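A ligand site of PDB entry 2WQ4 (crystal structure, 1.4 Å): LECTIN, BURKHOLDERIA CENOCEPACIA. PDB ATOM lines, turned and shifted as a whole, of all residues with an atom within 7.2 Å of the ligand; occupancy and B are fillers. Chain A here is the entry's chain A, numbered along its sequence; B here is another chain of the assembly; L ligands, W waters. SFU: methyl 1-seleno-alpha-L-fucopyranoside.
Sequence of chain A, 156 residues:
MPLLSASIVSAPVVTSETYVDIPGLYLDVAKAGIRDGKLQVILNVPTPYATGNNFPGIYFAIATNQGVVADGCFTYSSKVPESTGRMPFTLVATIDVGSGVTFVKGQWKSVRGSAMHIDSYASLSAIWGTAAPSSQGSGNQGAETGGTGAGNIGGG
Water W3 lies within hydrogen-bond range of O3 of the ligand (2.5 Å), OG of Ser 83 (2.7 Å) and O of Tyr 76 of chain B (2.7 Å).
Water W4 lies within hydrogen-bond range of O2 of the ligand (2.9 Å), OH of Tyr 59 of chain B (3.0 Å) and SG of Cys 73 of chain B (3.2 Å).
Water W1 bridges OH of Tyr 49 (3.0 Å) and NH2 of Arg 86 (3.3 Å).
Tyr 49 touches the ligand (CE1 to C6, 3.7 Å).
Ser 83 touches the ligand (OG to C4, 3.8 Å).
Gly 85 touches the ligand (CA to O4, 3.6 Å).
Hydrophobic or aromatic side chains within 4 Å of the ligand: Tyr 49.
Within 4 Å of the ligand: Tyr 49, Ser 83, Thr 84, Gly 85, Arg 86, Thr 75 of chain B and Arg 112 of chain B.
Along chain A the residues within 4 Å of the ligand span positions 49 to 86.
The side-chain hydroxyl (OG1) of Thr 75 of chain B is in hydrogen-bond range of the backbone NH (N) of Arg 86 (2.8 Å).
The guanidinium group (NH2) of Arg 112 of chain B lies within hydrogen-bond range of the backbone carbonyl oxygen (O) of Phe 55 of chain B, 2.8 Å away.
The guanidinium group (NH1) of Arg 86 lies within salt-bridge range of the side-chain carboxylate (OD1) of Asp 119 (2.8 Å).
The guanidinium group (NH1) of Arg 86 is in hydrogen-bond range of the backbone carbonyl oxygen (O) of Thr 47, at 2.9 Å.
O of Gly 85 is in hydrogen-bond range of OH of Tyr 76 of chain A, at 2.7 Å.
The backbone NH (N) of Gly 85 lies within hydrogen-bond range of the side-chain hydroxyl (OG) of Ser 77 of chain B, 3.0 Å away.
O of Tyr 49 sits at hydrogen-bond distance from N of His 117 (3.0 Å).
O of Ser 83 lies close to OG of Ser 77 of chain B (3.1 Å).
The side-chain hydroxyl (OG1) of Thr 75 of chain B sits at hydrogen-bond distance from an oxygen (O3) of the ligand (2.6 Å).
O4 of the ligand sits at hydrogen-bond distance from O of Thr 84, 2.8 Å away.
The guanidinium group of Arg 112 of chain B sits at hydrogen-bond distance from an oxygen (O2) of the ligand, 2.8 Å away.
The guanidinium group (NH2) of Arg 86 lies within hydrogen-bond range of an oxygen (O5) of the ligand, 2.9 Å away.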
ATOM      1  N   THR A  47       1.061 -15.571   0.774  1.00  0.00           N
ATOM      2  CA  THR A  47      -0.269 -15.616   1.439  1.00  0.00           C
ATOM      3  C   THR A  47      -1.051 -14.292   1.389  1.00  0.00           C
ATOM      4  O   THR A  47      -1.616 -13.879   2.391  1.00  0.00           O
ATOM      5  CB  THR A  47      -0.084 -16.069   2.908  1.00  0.00           C
ATOM      6  OG1 THR A  47       0.963 -17.050   2.965  1.00  0.00           O
ATOM      7  CG2 THR A  47      -1.332 -16.659   3.486  1.00  0.00           C
ATOM      8  N   PRO A  48      -1.119 -13.643   0.218  1.00  0.00           N
ATOM      9  CA  PRO A  48      -1.892 -12.422   0.152  1.00  0.00           C
ATOM     10  C   PRO A  48      -3.375 -12.681  -0.032  1.00  0.00           C
ATOM     11  O   PRO A  48      -3.801 -13.781  -0.410  1.00  0.00           O
ATOM     12  CB  PRO A  48      -1.362 -11.756  -1.128  1.00  0.00           C
ATOM     13  CG  PRO A  48      -1.129 -12.899  -2.022  1.00  0.00           C
ATOM     14  CD  PRO A  48      -0.626 -14.016  -1.128  1.00  0.00           C
ATOM     15  N   TYR A  49      -4.165 -11.663   0.225  1.00  0.00           N
ATOM     16  CA  TYR A  49      -5.535 -11.624  -0.237  1.00  0.00           C
ATOM     17  C   TYR A  49      -5.942 -10.231  -0.594  1.00  0.00           C
ATOM     18  O   TYR A  49      -5.286  -9.264  -0.169  1.00  0.00           O
ATOM     19  CB  TYR A  49      -6.504 -12.232   0.775  1.00  0.00           C
ATOM     20  CG  TYR A  49      -6.704 -11.510   2.056  1.00  0.00           C
ATOM     21  CD1 TYR A  49      -7.846 -10.763   2.297  1.00  0.00           C
ATOM     22  CD2 TYR A  49      -5.791 -11.654   3.099  1.00  0.00           C
ATOM     23  CE1 TYR A  49      -8.077 -10.147   3.509  1.00  0.00           C
ATOM     24  CE2 TYR A  49      -6.015 -11.054   4.337  1.00  0.00           C
ATOM     25  CZ  TYR A  49      -7.159 -10.312   4.546  1.00  0.00           C
ATOM     26  OH  TYR A  49      -7.417  -9.704   5.776  1.00  0.00           O
ATOM     27  N   THR A  51      -9.433  -7.570  -1.106  1.00  0.00           N
ATOM     28  CA  THR A  51     -10.843  -7.317  -0.841  1.00  0.00           C
ATOM     29  C   THR A  51     -11.305  -6.232  -1.787  1.00  0.00           C
ATOM     30  O   THR A  51     -10.558  -5.321  -2.112  1.00  0.00           O
ATOM     31  CB  THR A  51     -11.070  -6.910   0.634  1.00  0.00           C
ATOM     32  OG1 THR A  51     -10.317  -5.764   0.972  1.00  0.00           O
ATOM     33  CG2 THR A  51     -10.678  -8.076   1.540  1.00  0.00           C
ATOM     34  N   TYR A  76      -9.423 -13.069  -8.256  1.00  0.00           N
ATOM     35  CA  TYR A  76     -10.429 -14.058  -7.986  1.00  0.00           C
ATOM     36  C   TYR A  76     -11.329 -14.299  -9.175  1.00  0.00           C
ATOM     37  O   TYR A  76     -11.407 -13.482 -10.089  1.00  0.00           O
ATOM     38  CB  TYR A  76     -11.260 -13.652  -6.762  1.00  0.00           C
ATOM     39  CG  TYR A  76     -10.452 -13.531  -5.475  1.00  0.00           C
ATOM     40  CD1 TYR A  76      -9.884 -14.634  -4.888  1.00  0.00           C
ATOM     41  CD2 TYR A  76     -10.238 -12.301  -4.905  1.00  0.00           C
ATOM     42  CE1 TYR A  76      -9.149 -14.538  -3.734  1.00  0.00           C
ATOM     43  CE2 TYR A  76      -9.496 -12.187  -3.738  1.00  0.00           C
ATOM     44  CZ  TYR A  76      -8.923 -13.288  -3.173  1.00  0.00           C
ATOM     45  OH  TYR A  76      -8.165 -13.102  -2.027  1.00  0.00           O
ATOM     46  N   SER A  83     -15.461 -15.950   0.413  1.00  0.00           N
ATOM     47  CA  SER A  83     -14.381 -15.535   1.297  1.00  0.00           C
ATOM     48  C   SER A  83     -13.209 -15.246   0.373  1.00  0.00           C
ATOM     49  O   SER A  83     -12.993 -15.977  -0.615  1.00  0.00           O
ATOM     50  CB  SER A  83     -13.994 -16.669   2.266  1.00  0.00           C
ATOM     51  OG  SER A  83     -12.752 -16.410   2.923  1.00  0.00           O
ATOM     52  N   THR A  84     -12.442 -14.224   0.689  1.00  0.00           N
ATOM     53  CA  THR A  84     -11.272 -13.882  -0.115  1.00  0.00           C
ATOM     54  C   THR A  84     -10.079 -14.756   0.307  1.00  0.00           C
ATOM     55  O   THR A  84      -9.357 -14.483   1.281  1.00  0.00           O
ATOM     56  CB  THR A  84     -10.955 -12.391   0.043  1.00  0.00           C
ATOM     57  OG1 THR A  84     -10.700 -12.109   1.423  1.00  0.00           O
ATOM     58  CG2 THR A  84     -12.091 -11.539  -0.509  1.00  0.00           C
ATOM     59  N   GLY A  85      -9.919 -15.848  -0.424  1.00  0.00           N
ATOM     60  CA  GLY A  85      -8.899 -16.827  -0.079  1.00  0.00           C
ATOM     61  C   GLY A  85      -7.490 -16.369  -0.319  1.00  0.00           C
ATOM     62  O   GLY A  85      -7.231 -15.380  -1.031  1.00  0.00           O
ATOM     63  N   ARG A  86      -6.543 -17.109   0.254  1.00  0.00           N
ATOM     64  CA  ARG A  86      -5.144 -16.765   0.098  1.00  0.00           C
ATOM     65  C   ARG A  86      -4.585 -17.296  -1.198  1.00  0.00           C
ATOM     66  O   ARG A  86      -4.758 -18.464  -1.499  1.00  0.00           O
ATOM     67  CB  ARG A  86      -4.319 -17.274   1.278  1.00  0.00           C
ATOM     68  CG  ARG A  86      -4.849 -16.833   2.640  1.00  0.00           C
ATOM     69  CD  ARG A  86      -4.981 -15.302   2.723  1.00  0.00           C
ATOM     70  NE  ARG A  86      -5.420 -14.887   4.051  1.00  0.00           N
ATOM     71  CZ  ARG A  86      -4.693 -14.206   4.935  1.00  0.00           C
ATOM     72  NH1 ARG A  86      -3.443 -13.823   4.673  1.00  0.00           N
ATOM     73  NH2 ARG A  86      -5.223 -13.902   6.116  1.00  0.00           N
ATOM     74  N   MET A  87      -3.926 -16.441  -1.960  1.00  0.00           N
ATOM     75  CA  MET A  87      -3.543 -16.667  -3.355  1.00  0.00           C
ATOM     76  C   MET A  87      -2.047 -16.506  -3.541  1.00  0.00           C
ATOM     77  O   MET A  87      -1.574 -15.429  -3.871  1.00  0.00           O
ATOM     78  CB  MET A  87      -4.252 -15.633  -4.214  1.00  0.00           C
ATOM     79  CG  MET A  87      -5.764 -15.830  -4.236  1.00  0.00           C
ATOM     80  SD  MET A  87      -6.386 -17.382  -5.138  1.00  0.00           S
ATOM     81  CE  MET A  87      -6.766 -16.425  -6.762  1.00  0.00           C
ATOM     82  N   HIS A 117      -3.733  -6.962   1.033  1.00  0.00           N
ATOM     83  CA  HIS A 117      -3.439  -7.547   2.329  1.00  0.00           C
ATOM     84  C   HIS A 117      -2.288  -8.523   2.344  1.00  0.00           C
ATOM     85  O   HIS A 117      -2.335  -9.545   1.662  1.00  0.00           O
ATOM     86  CB  HIS A 117      -4.653  -8.288   2.894  1.00  0.00           C
ATOM     87  CG  HIS A 117      -5.906  -7.485   2.946  1.00  0.00           C
ATOM     88  ND1 HIS A 117      -6.441  -7.014   4.125  1.00  0.00           N
ATOM     89  CD2 HIS A 117      -6.745  -7.087   1.960  1.00  0.00           C
ATOM     90  CE1 HIS A 117      -7.563  -6.368   3.864  1.00  0.00           C
ATOM     91  NE2 HIS A 117      -7.767  -6.383   2.562  1.00  0.00           N
ATOM     92  N   ASP A 119      -0.379 -10.232   5.740  1.00  0.00           N
ATOM     93  CA  ASP A 119      -0.406 -10.323   7.198  1.00  0.00           C
ATOM     94  C   ASP A 119       0.453 -11.471   7.715  1.00  0.00           C
ATOM     95  O   ASP A 119       0.305 -11.919   8.850  1.00  0.00           O
ATOM     96  CB  ASP A 119      -1.861 -10.450   7.700  1.00  0.00           C
ATOM     97  CG  ASP A 119      -2.552 -11.702   7.221  1.00  0.00           C
ATOM     98  OD1 ASP A 119      -1.906 -12.618   6.657  1.00  0.00           O
ATOM     99  OD2 ASP A 119      -3.786 -11.793   7.449  1.00  0.00           O
ATOM    100  N   ASN B  54     -14.800 -26.558   5.307  1.00  0.00           N
ATOM    101  CA  ASN B  54     -14.852 -25.202   5.850  1.00  0.00           C
ATOM    102  C   ASN B  54     -13.703 -24.360   5.329  1.00  0.00           C
ATOM    103  O   ASN B  54     -12.748 -24.071   6.072  1.00  0.00           O
ATOM    104  CB  ASN B  54     -14.890 -25.200   7.386  1.00  0.00           C
ATOM    105  CG  ASN B  54     -15.214 -23.827   7.944  1.00  0.00           C
ATOM    106  OD1 ASN B  54     -15.938 -23.028   7.336  1.00  0.00           O
ATOM    107  ND2 ASN B  54     -14.710 -23.551   9.148  1.00  0.00           N
ATOM    108  N   PHE B  55     -13.840 -23.942   4.073  1.00  0.00           N
ATOM    109  CA  PHE B  55     -12.855 -23.088   3.381  1.00  0.00           C
ATOM    110  C   PHE B  55     -11.480 -23.746   3.484  1.00  0.00           C
ATOM    111  O   PHE B  55     -10.590 -23.282   4.203  1.00  0.00           O
ATOM    112  CB  PHE B  55     -12.821 -21.663   3.956  1.00  0.00           C
ATOM    113  CG  PHE B  55     -14.134 -20.913   3.833  1.00  0.00           C
ATOM    114  CD1 PHE B  55     -14.453 -20.229   2.663  1.00  0.00           C
ATOM    115  CD2 PHE B  55     -15.037 -20.917   4.867  1.00  0.00           C
ATOM    116  CE1 PHE B  55     -15.679 -19.540   2.542  1.00  0.00           C
ATOM    117  CE2 PHE B  55     -16.249 -20.210   4.745  1.00  0.00           C
ATOM    118  CZ  PHE B  55     -16.541 -19.536   3.597  1.00  0.00           C
ATOM    119  N   PRO B  56     -11.300 -24.864   2.763  1.00  0.00           N
ATOM    120  CA  PRO B  56     -10.084 -25.634   2.955  1.00  0.00           C
ATOM    121  C   PRO B  56      -8.805 -24.954   2.484  1.00  0.00           C
ATOM    122  O   PRO B  56      -8.839 -23.983   1.710  1.00  0.00           O
ATOM    123  CB  PRO B  56     -10.332 -26.887   2.121  1.00  0.00           C
ATOM    124  CG  PRO B  56     -11.804 -26.990   2.045  1.00  0.00           C
ATOM    125  CD  PRO B  56     -12.272 -25.603   1.942  1.00  0.00           C
ATOM    126  N   GLY B  57      -7.678 -25.461   2.968  1.00  0.00           N
ATOM    127  CA  GLY B  57      -6.381 -24.958   2.538  1.00  0.00           C
ATOM    128  C   GLY B  57      -5.256 -25.669   3.265  1.00  0.00           C
ATOM    129  O   GLY B  57      -5.494 -26.583   4.063  1.00  0.00           O
ATOM    130  N   TYR B  59      -1.258 -24.844   5.076  1.00  0.00           N
ATOM    131  CA  TYR B  59      -0.084 -24.067   5.444  1.00  0.00           C
ATOM    132  C   TYR B  59       1.156 -24.874   5.116  1.00  0.00           C
ATOM    133  O   TYR B  59       1.193 -26.085   5.372  1.00  0.00           O
ATOM    134  CB  TYR B  59      -0.005 -23.829   6.955  1.00  0.00           C
ATOM    135  CG  TYR B  59      -1.041 -22.972   7.596  1.00  0.00           C
ATOM    136  CD1 TYR B  59      -0.930 -21.595   7.589  1.00  0.00           C
ATOM    137  CD2 TYR B  59      -2.168 -23.542   8.205  1.00  0.00           C
ATOM    138  CE1 TYR B  59      -1.925 -20.794   8.193  1.00  0.00           C
ATOM    139  CE2 TYR B  59      -3.134 -22.763   8.838  1.00  0.00           C
ATOM    140  CZ  TYR B  59      -3.016 -21.397   8.826  1.00  0.00           C
ATOM    141  OH  TYR B  59      -4.015 -20.649   9.441  1.00  0.00           O
ATOM    142  N   CYS B  73       0.283 -19.954   3.336  1.00  0.00           N
ATOM    143  CA  CYS B  73      -0.762 -20.926   2.968  1.00  0.00           C
ATOM    144  C   CYS B  73      -1.473 -20.512   1.698  1.00  0.00           C
ATOM    145  O   CYS B  73      -1.414 -19.349   1.282  1.00  0.00           O
ATOM    146  CB  CYS B  73      -1.805 -21.058   4.092  1.00  0.00           C
ATOM    147  SG  CYS B  73      -3.003 -19.686   4.333  1.00  0.00           S
ATOM    148  N   PHE B  74      -2.186 -21.460   1.103  1.00  0.00           N
ATOM    149  CA  PHE B  74      -3.285 -21.171   0.195  1.00  0.00           C
ATOM    150  C   PHE B  74      -4.575 -21.592   0.878  1.00  0.00           C
ATOM    151  O   PHE B  74      -4.599 -22.536   1.688  1.00  0.00           O
ATOM    152  CB  PHE B  74      -3.171 -21.851  -1.167  1.00  0.00           C
ATOM    153  CG  PHE B  74      -3.481 -23.305  -1.169  1.00  0.00           C
ATOM    154  CD1 PHE B  74      -4.787 -23.763  -1.272  1.00  0.00           C
ATOM    155  CD2 PHE B  74      -2.472 -24.257  -1.050  1.00  0.00           C
ATOM    156  CE1 PHE B  74      -5.058 -25.130  -1.298  1.00  0.00           C
ATOM    157  CE2 PHE B  74      -2.743 -25.606  -1.051  1.00  0.00           C
ATOM    158  CZ  PHE B  74      -4.026 -26.025  -1.173  1.00  0.00           C
ATOM    159  N   THR B  75      -5.654 -20.883   0.554  1.00  0.00           N
ATOM    160  CA  THR B  75      -7.006 -21.283   0.930  1.00  0.00           C
ATOM    161  C   THR B  75      -7.969 -21.074  -0.255  1.00  0.00           C
ATOM    162  O   THR B  75      -7.776 -20.166  -1.083  1.00  0.00           O
ATOM    163  CB  THR B  75      -7.545 -20.549   2.159  1.00  0.00           C
ATOM    164  OG1 THR B  75      -7.571 -19.143   1.900  1.00  0.00           O
ATOM    165  CG2 THR B  75      -6.680 -20.834   3.377  1.00  0.00           C
ATOM    166  N   TYR B  76      -9.018 -21.898  -0.308  1.00  0.00           N
ATOM    167  CA  TYR B  76     -10.075 -21.682  -1.278  1.00  0.00           C
ATOM    168  C   TYR B  76     -10.985 -20.530  -0.846  1.00  0.00           C
ATOM    169  O   TYR B  76     -11.045 -20.165   0.331  1.00  0.00           O
ATOM    170  CB  TYR B  76     -10.889 -22.938  -1.495  1.00  0.00           C
ATOM    171  CG  TYR B  76     -10.066 -24.092  -2.051  1.00  0.00           C
ATOM    172  CD1 TYR B  76      -9.570 -24.060  -3.337  1.00  0.00           C
ATOM    173  CD2 TYR B  76      -9.800 -25.202  -1.253  1.00  0.00           C
ATOM    174  CE1 TYR B  76      -8.816 -25.137  -3.822  1.00  0.00           C
ATOM    175  CE2 TYR B  76      -9.062 -26.250  -1.705  1.00  0.00           C
ATOM    176  CZ  TYR B  76      -8.551 -26.213  -2.983  1.00  0.00           C
ATOM    177  OH  TYR B  76      -7.821 -27.266  -3.455  1.00  0.00           O
ATOM    178  N   SER B  77     -11.720 -20.015  -1.805  1.00  0.00           N
ATOM    179  CA  SER B  77     -12.604 -18.874  -1.598  1.00  0.00           C
ATOM    180  C   SER B  77     -14.076 -19.257  -1.481  1.00  0.00           C
ATOM    181  O   SER B  77     -14.952 -18.368  -1.527  1.00  0.00           O
ATOM    182  CB  SER B  77     -12.419 -17.918  -2.777  1.00  0.00           C
ATOM    183  OG  SER B  77     -11.164 -17.247  -2.705  1.00  0.00           O
ATOM    184  N   VAL B 111      -5.257 -26.244   7.190  1.00  0.00           N
ATOM    185  CA  VAL B 111      -6.150 -25.124   7.471  1.00  0.00           C
ATOM    186  C   VAL B 111      -7.534 -25.703   7.783  1.00  0.00           C
ATOM    187  O   VAL B 111      -8.073 -26.482   6.989  1.00  0.00           O
ATOM    188  CB  VAL B 111      -6.255 -24.114   6.298  1.00  0.00           C
ATOM    189  CG1 VAL B 111      -7.269 -23.018   6.644  1.00  0.00           C
ATOM    190  CG2 VAL B 111      -4.892 -23.496   5.970  1.00  0.00           C
ATOM    191  N   ARG B 112      -8.064 -25.399   8.964  1.00  0.00           N
ATOM    192  CA  ARG B 112      -9.434 -25.802   9.322  1.00  0.00           C
ATOM    193  C   ARG B 112      -9.703 -27.286   9.054  1.00  0.00           C
ATOM    194  O   ARG B 112     -10.710 -27.646   8.440  1.00  0.00           O
ATOM    195  CB  ARG B 112     -10.466 -24.880   8.635  1.00  0.00           C
ATOM    196  CG  ARG B 112     -10.404 -23.452   9.224  1.00  0.00           C
ATOM    197  CD  ARG B 112     -11.397 -22.526   8.525  1.00  0.00           C
ATOM    198  NE  ARG B 112     -10.950 -22.175   7.189  1.00  0.00           N
ATOM    199  CZ  ARG B 112     -10.130 -21.168   6.874  1.00  0.00           C
ATOM    200  NH1 ARG B 112      -9.623 -20.361   7.802  1.00  0.00           N
ATOM    201  NH2 ARG B 112      -9.825 -20.982   5.608  1.00  0.00           N
HETATM  202  C1  SFU L   1      -7.747 -16.372   6.683  1.00  0.00           C
HETATM  203  C2  SFU L   1      -7.808 -17.516   5.687  1.00  0.00           C
HETATM  204  C3  SFU L   1      -9.095 -17.426   4.856  1.00  0.00           C
HETATM  205  C4  SFU L   1      -9.200 -16.054   4.207  1.00  0.00           C
HETATM  206  C5  SFU L   1      -9.121 -14.934   5.267  1.00  0.00           C
HETATM  207  C6  SFU L   1      -9.132 -13.533   4.691  1.00  0.00           C
HETATM  208  O2  SFU L   1      -7.765 -18.778   6.381  1.00  0.00           O
HETATM  209  O3  SFU L   1      -9.110 -18.487   3.919  1.00  0.00           O
HETATM  210  O4  SFU L   1      -8.104 -15.916   3.294  1.00  0.00           O
HETATM  211  O5  SFU L   1      -7.890 -15.095   6.034  1.00  0.00           O
HETATM  212  CM  SFU L   1      -8.689 -14.942   8.993  1.00  0.00           C
HETATM  213 SE   SFU L   1      -9.095 -16.632   8.130  1.00  0.00          SE
HETATM  214  O   HOH W   1      -7.441 -11.994   7.745  1.00  0.00           O
HETATM  215  O   HOH W   2     -10.289 -12.126   7.708  1.00  0.00           O
HETATM  216  O   HOH W   3     -11.261 -18.629   2.577  1.00  0.00           O
HETATM  217  O   HOH W   4      -5.022 -19.503   6.801  1.00  0.00           O
